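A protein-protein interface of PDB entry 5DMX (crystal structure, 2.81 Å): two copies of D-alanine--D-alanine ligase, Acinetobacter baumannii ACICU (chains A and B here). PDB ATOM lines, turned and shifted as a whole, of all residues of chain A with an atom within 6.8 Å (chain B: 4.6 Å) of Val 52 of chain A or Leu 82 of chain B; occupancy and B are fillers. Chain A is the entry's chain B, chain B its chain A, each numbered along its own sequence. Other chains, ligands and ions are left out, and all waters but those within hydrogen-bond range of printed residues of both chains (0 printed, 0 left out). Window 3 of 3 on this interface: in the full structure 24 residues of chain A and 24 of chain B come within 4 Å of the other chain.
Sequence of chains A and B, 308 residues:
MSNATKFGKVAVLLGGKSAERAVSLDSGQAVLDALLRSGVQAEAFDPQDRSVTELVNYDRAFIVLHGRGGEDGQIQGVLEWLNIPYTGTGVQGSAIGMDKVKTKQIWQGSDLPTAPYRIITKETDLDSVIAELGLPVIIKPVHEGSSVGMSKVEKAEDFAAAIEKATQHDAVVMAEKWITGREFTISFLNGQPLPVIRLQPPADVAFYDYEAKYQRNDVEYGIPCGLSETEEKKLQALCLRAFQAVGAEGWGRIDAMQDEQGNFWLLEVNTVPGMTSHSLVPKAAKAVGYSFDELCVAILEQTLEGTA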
ATOM      1  N   LEU A  13      15.054  33.491  26.786  1.00  0.00           N
ATOM      2  CA  LEU A  13      16.266  32.725  27.096  1.00  0.00           C
ATOM      3  C   LEU A  13      17.136  33.583  27.994  1.00  0.00           C
ATOM      4  O   LEU A  13      17.527  34.679  27.599  1.00  0.00           O
ATOM      5  CB  LEU A  13      17.050  32.349  25.810  1.00  0.00           C
ATOM      6  CG  LEU A  13      16.923  31.011  25.027  1.00  0.00           C
ATOM      7  CD1 LEU A  13      16.234  29.915  25.813  1.00  0.00           C
ATOM      8  CD2 LEU A  13      16.221  31.191  23.692  1.00  0.00           C
ATOM      9  N   LYS A  17      25.191  29.672  30.673  1.00  0.00           N
ATOM     10  CA  LYS A  17      26.408  29.023  31.153  1.00  0.00           C
ATOM     11  C   LYS A  17      27.608  29.960  31.409  1.00  0.00           C
ATOM     12  O   LYS A  17      28.527  29.597  32.145  1.00  0.00           O
ATOM     13  CB  LYS A  17      26.790  27.895  30.176  1.00  0.00           C
ATOM     14  CG  LYS A  17      27.185  28.299  28.761  1.00  0.00           C
ATOM     15  CD  LYS A  17      27.014  27.101  27.801  1.00  0.00           C
ATOM     16  CE  LYS A  17      28.197  26.835  26.895  1.00  0.00           C
ATOM     17  NZ  LYS A  17      27.804  26.007  25.729  1.00  0.00           N
ATOM     18  N   PHE A  45      13.279  30.701  30.324  1.00  0.00           N
ATOM     19  CA  PHE A  45      13.966  29.479  29.931  1.00  0.00           C
ATOM     20  C   PHE A  45      15.442  29.674  30.213  1.00  0.00           C
ATOM     21  O   PHE A  45      16.094  30.457  29.530  1.00  0.00           O
ATOM     22  CB  PHE A  45      13.726  29.235  28.443  1.00  0.00           C
ATOM     23  CG  PHE A  45      13.972  27.818  28.007  1.00  0.00           C
ATOM     24  CD1 PHE A  45      15.212  27.211  28.172  1.00  0.00           C
ATOM     25  CD2 PHE A  45      12.965  27.097  27.396  1.00  0.00           C
ATOM     26  CE1 PHE A  45      15.427  25.914  27.754  1.00  0.00           C
ATOM     27  CE2 PHE A  45      13.181  25.802  26.982  1.00  0.00           C
ATOM     28  CZ  PHE A  45      14.410  25.212  27.159  1.00  0.00           C
ATOM     29  N   PRO A  47      18.878  27.884  29.947  1.00  0.00           N
ATOM     30  CA  PRO A  47      19.428  26.670  29.360  1.00  0.00           C
ATOM     31  C   PRO A  47      20.423  25.923  30.219  1.00  0.00           C
ATOM     32  O   PRO A  47      20.777  24.808  29.872  1.00  0.00           O
ATOM     33  CB  PRO A  47      20.103  27.148  28.070  1.00  0.00           C
ATOM     34  CG  PRO A  47      19.635  28.532  27.849  1.00  0.00           C
ATOM     35  CD  PRO A  47      19.293  29.074  29.196  1.00  0.00           C
ATOM     36  N   ARG A  50      17.396  23.942  32.177  1.00  0.00           N
ATOM     37  CA  ARG A  50      16.449  23.244  31.321  1.00  0.00           C
ATOM     38  C   ARG A  50      17.151  22.837  30.039  1.00  0.00           C
ATOM     39  O   ARG A  50      17.735  23.682  29.370  1.00  0.00           O
ATOM     40  CB  ARG A  50      15.291  24.169  30.946  1.00  0.00           C
ATOM     41  CG  ARG A  50      14.008  23.919  31.713  1.00  0.00           C
ATOM     42  CD  ARG A  50      12.839  23.553  30.802  1.00  0.00           C
ATOM     43  NE  ARG A  50      12.054  24.724  30.401  1.00  0.00           N
ATOM     44  CZ  ARG A  50      10.857  24.681  29.810  1.00  0.00           C
ATOM     45  NH1 ARG A  50      10.261  23.527  29.524  1.00  0.00           N
ATOM     46  NH2 ARG A  50      10.251  25.810  29.494  1.00  0.00           N
ATOM     47  N   SER A  51      17.072  21.560  29.672  1.00  0.00           N
ATOM     48  CA  SER A  51      17.652  21.113  28.409  1.00  0.00           C
ATOM     49  C   SER A  51      17.033  21.889  27.252  1.00  0.00           C
ATOM     50  O   SER A  51      15.812  22.061  27.211  1.00  0.00           O
ATOM     51  CB  SER A  51      17.424  19.625  28.195  1.00  0.00           C
ATOM     52  OG  SER A  51      17.663  19.286  26.843  1.00  0.00           O
ATOM     53  N   VAL A  52      17.878  22.342  26.326  1.00  0.00           N
ATOM     54  CA  VAL A  52      17.414  23.050  25.114  1.00  0.00           C
ATOM     55  C   VAL A  52      16.409  22.267  24.283  1.00  0.00           C
ATOM     56  O   VAL A  52      15.684  22.862  23.482  1.00  0.00           O
ATOM     57  CB  VAL A  52      18.572  23.506  24.178  1.00  0.00           C
ATOM     58  CG1 VAL A  52      19.311  24.696  24.765  1.00  0.00           C
ATOM     59  CG2 VAL A  52      19.543  22.381  23.870  1.00  0.00           C
ATOM     60  N   THR A  53      16.374  20.942  24.464  1.00  0.00           N
ATOM     61  CA  THR A  53      15.392  20.062  23.800  1.00  0.00           C
ATOM     62  C   THR A  53      13.940  20.528  24.003  1.00  0.00           C
ATOM     63  O   THR A  53      13.124  20.470  23.075  1.00  0.00           O
ATOM     64  CB  THR A  53      15.509  18.603  24.288  1.00  0.00           C
ATOM     65  OG1 THR A  53      15.277  18.533  25.695  1.00  0.00           O
ATOM     66  CG2 THR A  53      16.899  18.007  23.972  1.00  0.00           C
ATOM     67  N   GLU A  54      13.642  21.035  25.201  1.00  0.00           N
ATOM     68  CA  GLU A  54      12.305  21.533  25.517  1.00  0.00           C
ATOM     69  C   GLU A  54      11.929  22.845  24.806  1.00  0.00           C
ATOM     70  O   GLU A  54      10.763  23.258  24.856  1.00  0.00           O
ATOM     71  CB  GLU A  54      12.129  21.656  27.033  1.00  0.00           C
ATOM     72  CG  GLU A  54      12.147  20.324  27.756  1.00  0.00           C
ATOM     73  CD  GLU A  54      12.219  20.440  29.273  1.00  0.00           C
ATOM     74  OE1 GLU A  54      11.232  20.927  29.866  1.00  0.00           O
ATOM     75  OE2 GLU A  54      13.251  20.031  29.872  1.00  0.00           O
ATOM     76  N   LEU A  55      12.884  23.505  24.149  1.00  0.00           N
ATOM     77  CA  LEU A  55      12.564  24.700  23.342  1.00  0.00           C
ATOM     78  C   LEU A  55      11.504  24.439  22.289  1.00  0.00           C
ATOM     79  O   LEU A  55      10.782  25.355  21.865  1.00  0.00           O
ATOM     80  CB  LEU A  55      13.806  25.266  22.657  1.00  0.00           C
ATOM     81  CG  LEU A  55      14.643  26.195  23.533  1.00  0.00           C
ATOM     82  CD1 LEU A  55      16.090  26.228  23.074  1.00  0.00           C
ATOM     83  CD2 LEU A  55      14.041  27.590  23.504  1.00  0.00           C
ATOM     84  N   VAL A  56      11.406  23.181  21.885  1.00  0.00           N
ATOM     85  CA  VAL A  56      10.434  22.768  20.880  1.00  0.00           C
ATOM     86  C   VAL A  56       8.975  23.091  21.279  1.00  0.00           C
ATOM     87  O   VAL A  56       8.134  23.297  20.408  1.00  0.00           O
ATOM     88  CB  VAL A  56      10.652  21.282  20.503  1.00  0.00           C
ATOM     89  CG1 VAL A  56      10.144  20.358  21.601  1.00  0.00           C
ATOM     90  CG2 VAL A  56      10.025  20.972  19.155  1.00  0.00           C
ATOM     91  N   ILE A  75      23.492  29.126  20.655  1.00  0.00           N
ATOM     92  CA  ILE A  75      22.045  29.018  20.850  1.00  0.00           C
ATOM     93  C   ILE A  75      21.303  29.343  19.548  1.00  0.00           C
ATOM     94  O   ILE A  75      20.210  28.803  19.329  1.00  0.00           O
ATOM     95  CB  ILE A  75      21.495  29.893  22.026  1.00  0.00           C
ATOM     96  CG1 ILE A  75      20.099  29.420  22.485  1.00  0.00           C
ATOM     97  CG2 ILE A  75      21.440  31.387  21.669  1.00  0.00           C
ATOM     98  CD1 ILE A  75      20.087  28.070  23.159  1.00  0.00           C
ATOM     99  N   VAL A  78      20.970  26.196  17.640  1.00  0.00           N
ATOM    100  CA  VAL A  78      19.940  25.233  18.055  1.00  0.00           C
ATOM    101  C   VAL A  78      18.583  25.722  17.605  1.00  0.00           C
ATOM    102  O   VAL A  78      17.739  24.931  17.203  1.00  0.00           O
ATOM    103  CB  VAL A  78      19.940  24.802  19.554  1.00  0.00           C
ATOM    104  CG1 VAL A  78      21.295  24.974  20.218  1.00  0.00           C
ATOM    105  CG2 VAL A  78      18.870  25.486  20.365  1.00  0.00           C
ATOM    106  N   LEU A  82      15.737  23.870  15.246  1.00  0.00           N
ATOM    107  CA  LEU A  82      14.392  23.582  15.741  1.00  0.00           C
ATOM    108  C   LEU A  82      13.350  24.404  15.022  1.00  0.00           C
ATOM    109  O   LEU A  82      12.169  24.284  15.314  1.00  0.00           O
ATOM    110  CB  LEU A  82      14.351  23.776  17.238  1.00  0.00           C
ATOM    111  CG  LEU A  82      14.803  22.602  18.130  1.00  0.00           C
ATOM    112  CD1 LEU A  82      15.832  21.686  17.502  1.00  0.00           C
ATOM    113  CD2 LEU A  82      15.330  23.092  19.485  1.00  0.00           C
ATOM    114  N   ILE A  84      12.633  27.597  15.093  1.00  0.00           N
ATOM    115  CA  ILE A  84      12.021  28.552  16.028  1.00  0.00           C
ATOM    116  C   ILE A  84      12.593  29.953  15.738  1.00  0.00           C
ATOM    117  O   ILE A  84      13.781  30.173  15.974  1.00  0.00           O
ATOM    118  CB  ILE A  84      12.368  28.140  17.474  1.00  0.00           C
ATOM    119  CG1 ILE A  84      11.766  26.773  17.777  1.00  0.00           C
ATOM    120  CG2 ILE A  84      11.873  29.181  18.481  1.00  0.00           C
ATOM    121  CD1 ILE A  84      12.077  26.223  19.164  1.00  0.00           C
ATOM    122  N   VAL B  52      17.522  16.297  16.636  1.00  0.00           N
ATOM    123  CA  VAL B  52      18.877  16.519  17.172  1.00  0.00           C
ATOM    124  C   VAL B  52      18.977  16.304  18.663  1.00  0.00           C
ATOM    125  O   VAL B  52      20.076  16.096  19.179  1.00  0.00           O
ATOM    126  CB  VAL B  52      19.457  17.921  16.843  1.00  0.00           C
ATOM    127  CG1 VAL B  52      19.889  18.007  15.380  1.00  0.00           C
ATOM    128  CG2 VAL B  52      18.485  19.035  17.181  1.00  0.00           C
ATOM    129  N   LEU B  55      20.955  13.354  19.884  1.00  0.00           N
ATOM    130  CA  LEU B  55      22.421  13.403  19.846  1.00  0.00           C
ATOM    131  C   LEU B  55      23.053  13.179  21.202  1.00  0.00           C
ATOM    132  O   LEU B  55      24.212  12.752  21.306  1.00  0.00           O
ATOM    133  CB  LEU B  55      22.927  14.732  19.266  1.00  0.00           C
ATOM    134  CG  LEU B  55      22.971  14.773  17.739  1.00  0.00           C
ATOM    135  CD1 LEU B  55      22.875  16.192  17.214  1.00  0.00           C
ATOM    136  CD2 LEU B  55      24.250  14.110  17.249  1.00  0.00           C
ATOM    137  N   VAL B  78      24.557  23.274  17.869  1.00  0.00           N
ATOM    138  CA  VAL B  78      23.841  22.325  18.738  1.00  0.00           C
ATOM    139  C   VAL B  78      24.833  21.415  19.454  1.00  0.00           C
ATOM    140  O   VAL B  78      24.640  21.093  20.619  1.00  0.00           O
ATOM    141  CB  VAL B  78      22.673  21.518  18.098  1.00  0.00           C
ATOM    142  CG1 VAL B  78      22.084  22.200  16.878  1.00  0.00           C
ATOM    143  CG2 VAL B  78      23.053  20.090  17.778  1.00  0.00           C
ATOM    144  N   LEU B  79      25.895  21.029  18.771  1.00  0.00           N
ATOM    145  CA  LEU B  79      26.884  20.162  19.379  1.00  0.00           C
ATOM    146  C   LEU B  79      27.620  20.865  20.501  1.00  0.00           C
ATOM    147  O   LEU B  79      27.928  20.231  21.504  1.00  0.00           O
ATOM    148  CB  LEU B  79      27.848  19.578  18.324  1.00  0.00           C
ATOM    149  CG  LEU B  79      27.190  18.643  17.296  1.00  0.00           C
ATOM    150  CD1 LEU B  79      28.150  18.353  16.154  1.00  0.00           C
ATOM    151  CD2 LEU B  79      26.713  17.336  17.929  1.00  0.00           C
ATOM    152  N   GLU B  80      27.887  22.159  20.359  1.00  0.00           N
ATOM    153  CA  GLU B  80      28.531  22.933  21.439  1.00  0.00           C
ATOM    154  C   GLU B  80      27.611  22.960  22.665  1.00  0.00           C
ATOM    155  O   GLU B  80      28.048  22.666  23.768  1.00  0.00           O
ATOM    156  CB  GLU B  80      28.863  24.375  21.017  1.00  0.00           C
ATOM    157  CG  GLU B  80      29.877  24.528  19.894  1.00  0.00           C
ATOM    158  CD  GLU B  80      31.311  24.318  20.308  1.00  0.00           C
ATOM    159  OE1 GLU B  80      31.557  23.747  21.388  1.00  0.00           O
ATOM    160  OE2 GLU B  80      32.208  24.703  19.529  1.00  0.00           O
ATOM    161  N   TRP B  81      26.331  23.238  22.452  1.00  0.00           N
ATOM    162  CA  TRP B  81      25.375  23.221  23.543  1.00  0.00           C
ATOM    163  C   TRP B  81      25.109  21.866  24.186  1.00  0.00           C
ATOM    164  O   TRP B  81      24.705  21.833  25.341  1.00  0.00           O
ATOM    165  CB  TRP B  81      24.030  23.846  23.180  1.00  0.00           C
ATOM    166  CG  TRP B  81      23.602  24.660  24.281  1.00  0.00           C
ATOM    167  CD1 TRP B  81      23.145  24.241  25.510  1.00  0.00           C
ATOM    168  CD2 TRP B  81      23.679  26.054  24.342  1.00  0.00           C
ATOM    169  NE1 TRP B  81      22.902  25.320  26.320  1.00  0.00           N
ATOM    170  CE2 TRP B  81      23.220  26.448  25.628  1.00  0.00           C
ATOM    171  CE3 TRP B  81      24.063  27.018  23.427  1.00  0.00           C
ATOM    172  CZ2 TRP B  81      23.151  27.748  26.014  1.00  0.00           C
ATOM    173  CZ3 TRP B  81      23.988  28.292  23.797  1.00  0.00           C
ATOM    174  CH2 TRP B  81      23.535  28.673  25.094  1.00  0.00           C
ATOM    175  N   LEU B  82      25.343  20.765  23.481  1.00  0.00           N
ATOM    176  CA  LEU B  82      25.218  19.444  24.081  1.00  0.00           C
ATOM    177  C   LEU B  82      26.565  18.892  24.598  1.00  0.00           C
ATOM    178  O   LEU B  82      26.604  17.804  25.131  1.00  0.00           O
ATOM    179  CB  LEU B  82      24.573  18.513  23.095  1.00  0.00           C
ATOM    180  CG  LEU B  82      23.049  18.534  23.014  1.00  0.00           C
ATOM    181  CD1 LEU B  82      22.399  19.846  23.383  1.00  0.00           C
ATOM    182  CD2 LEU B  82      22.556  18.100  21.623  1.00  0.00           C
ATOM    183  N   ASN B  83      27.641  19.668  24.511  1.00  0.00           N
ATOM    184  CA  ASN B  83      28.977  19.257  24.971  1.00  0.00           C
ATOM    185  C   ASN B  83      29.523  17.980  24.331  1.00  0.00           C
ATOM    186  O   ASN B  83      30.183  17.182  25.004  1.00  0.00           O
ATOM    187  CB  ASN B  83      29.029  19.165  26.491  1.00  0.00           C
ATOM    188  CG  ASN B  83      28.707  20.482  27.132  1.00  0.00           C
ATOM    189  OD1 ASN B  83      27.590  20.697  27.599  1.00  0.00           O
ATOM    190  ND2 ASN B  83      29.668  21.404  27.101  1.00  0.00           N
ATOM    191  N   ILE B  84      29.268  17.841  23.031  1.00  0.00           N
ATOM    192  CA  ILE B  84      29.662  16.693  22.240  1.00  0.00           C
ATOM    193  C   ILE B  84      30.773  17.142  21.282  1.00  0.00           C
ATOM    194  O   ILE B  84      30.504  17.913  20.382  1.00  0.00           O
ATOM    195  CB  ILE B  84      28.443  16.197  21.435  1.00  0.00           C
ATOM    196  CG1 ILE B  84      27.338  15.722  22.387  1.00  0.00           C
ATOM    197  CG2 ILE B  84      28.839  15.070  20.492  1.00  0.00           C
ATOM    198  CD1 ILE B  84      26.057  15.244  21.724  1.00  0.00           C
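Val 52 of chain A touches Leu 82 of chain B, and with the chains exchanged Leu 82 of chain A touches Val 52 of chain B. Val 78 of chain B touches its own counterpart, Val 78 of chain A. Positions printed for both chains: 52, 55, 78, 82 and 84.
Of chain B, only Trp 81 and Leu 82 come within 4 Å of Val 52 of chain A. Val 56 of chain A touches none of the printed residues of chain B. Of the printed residues of chain B, Val 78 of chain A touches Val 78 (3.9 Å). Printed residues of chain B within 4 Å of Leu 82 of chain A: Val 52 (3.8 Å). Printed residues of chain A within 4 Å of Val 52 of chain B: Leu 82. Printed residues of chain A within 4 Å of Trp 81 of chain B: Pro 47, Val 52 and Ile 75. Of chain A, only Val 52 (3.8 Å) comes within 4 Å of Leu 82 of chain B. The nearest printed residue of chain A that does not touch Glu 80 of chain B is Val 78 of chain A (7.1 Å).
Glu 80 of chain B touches Lys 17 of chain A. Trp 81 of chain B touches Pro 47 of chain A. CG1 of Val 52 of chain A touches CD1 of Trp 81 of chain B (3.9 Å). Leu 82 of chain B touches Val 52 of chain A. Trp 81 of chain B touches Ile 75 of chain A (CZ3 to N, 3.3 Å). Val 78 of chain A touches Val 78 of chain B (CA to CG1, 3.9 Å). CG2 of Val 52 of chain B touches CD1 of Leu 82 of chain A, 3.8 Å away.
Of the 15 printed residues of chain A, 6 touch a printed residue of chain B. Printed residues of chain A that touch a printed residue of chain B: Lys 17, Pro 47, Val 52, Ile 75, Val 78 and Leu 82. Among the printed residues, no Asp or Glu carboxylate lies within 4 Å of a Lys or Arg side-chain nitrogen of the other chain.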
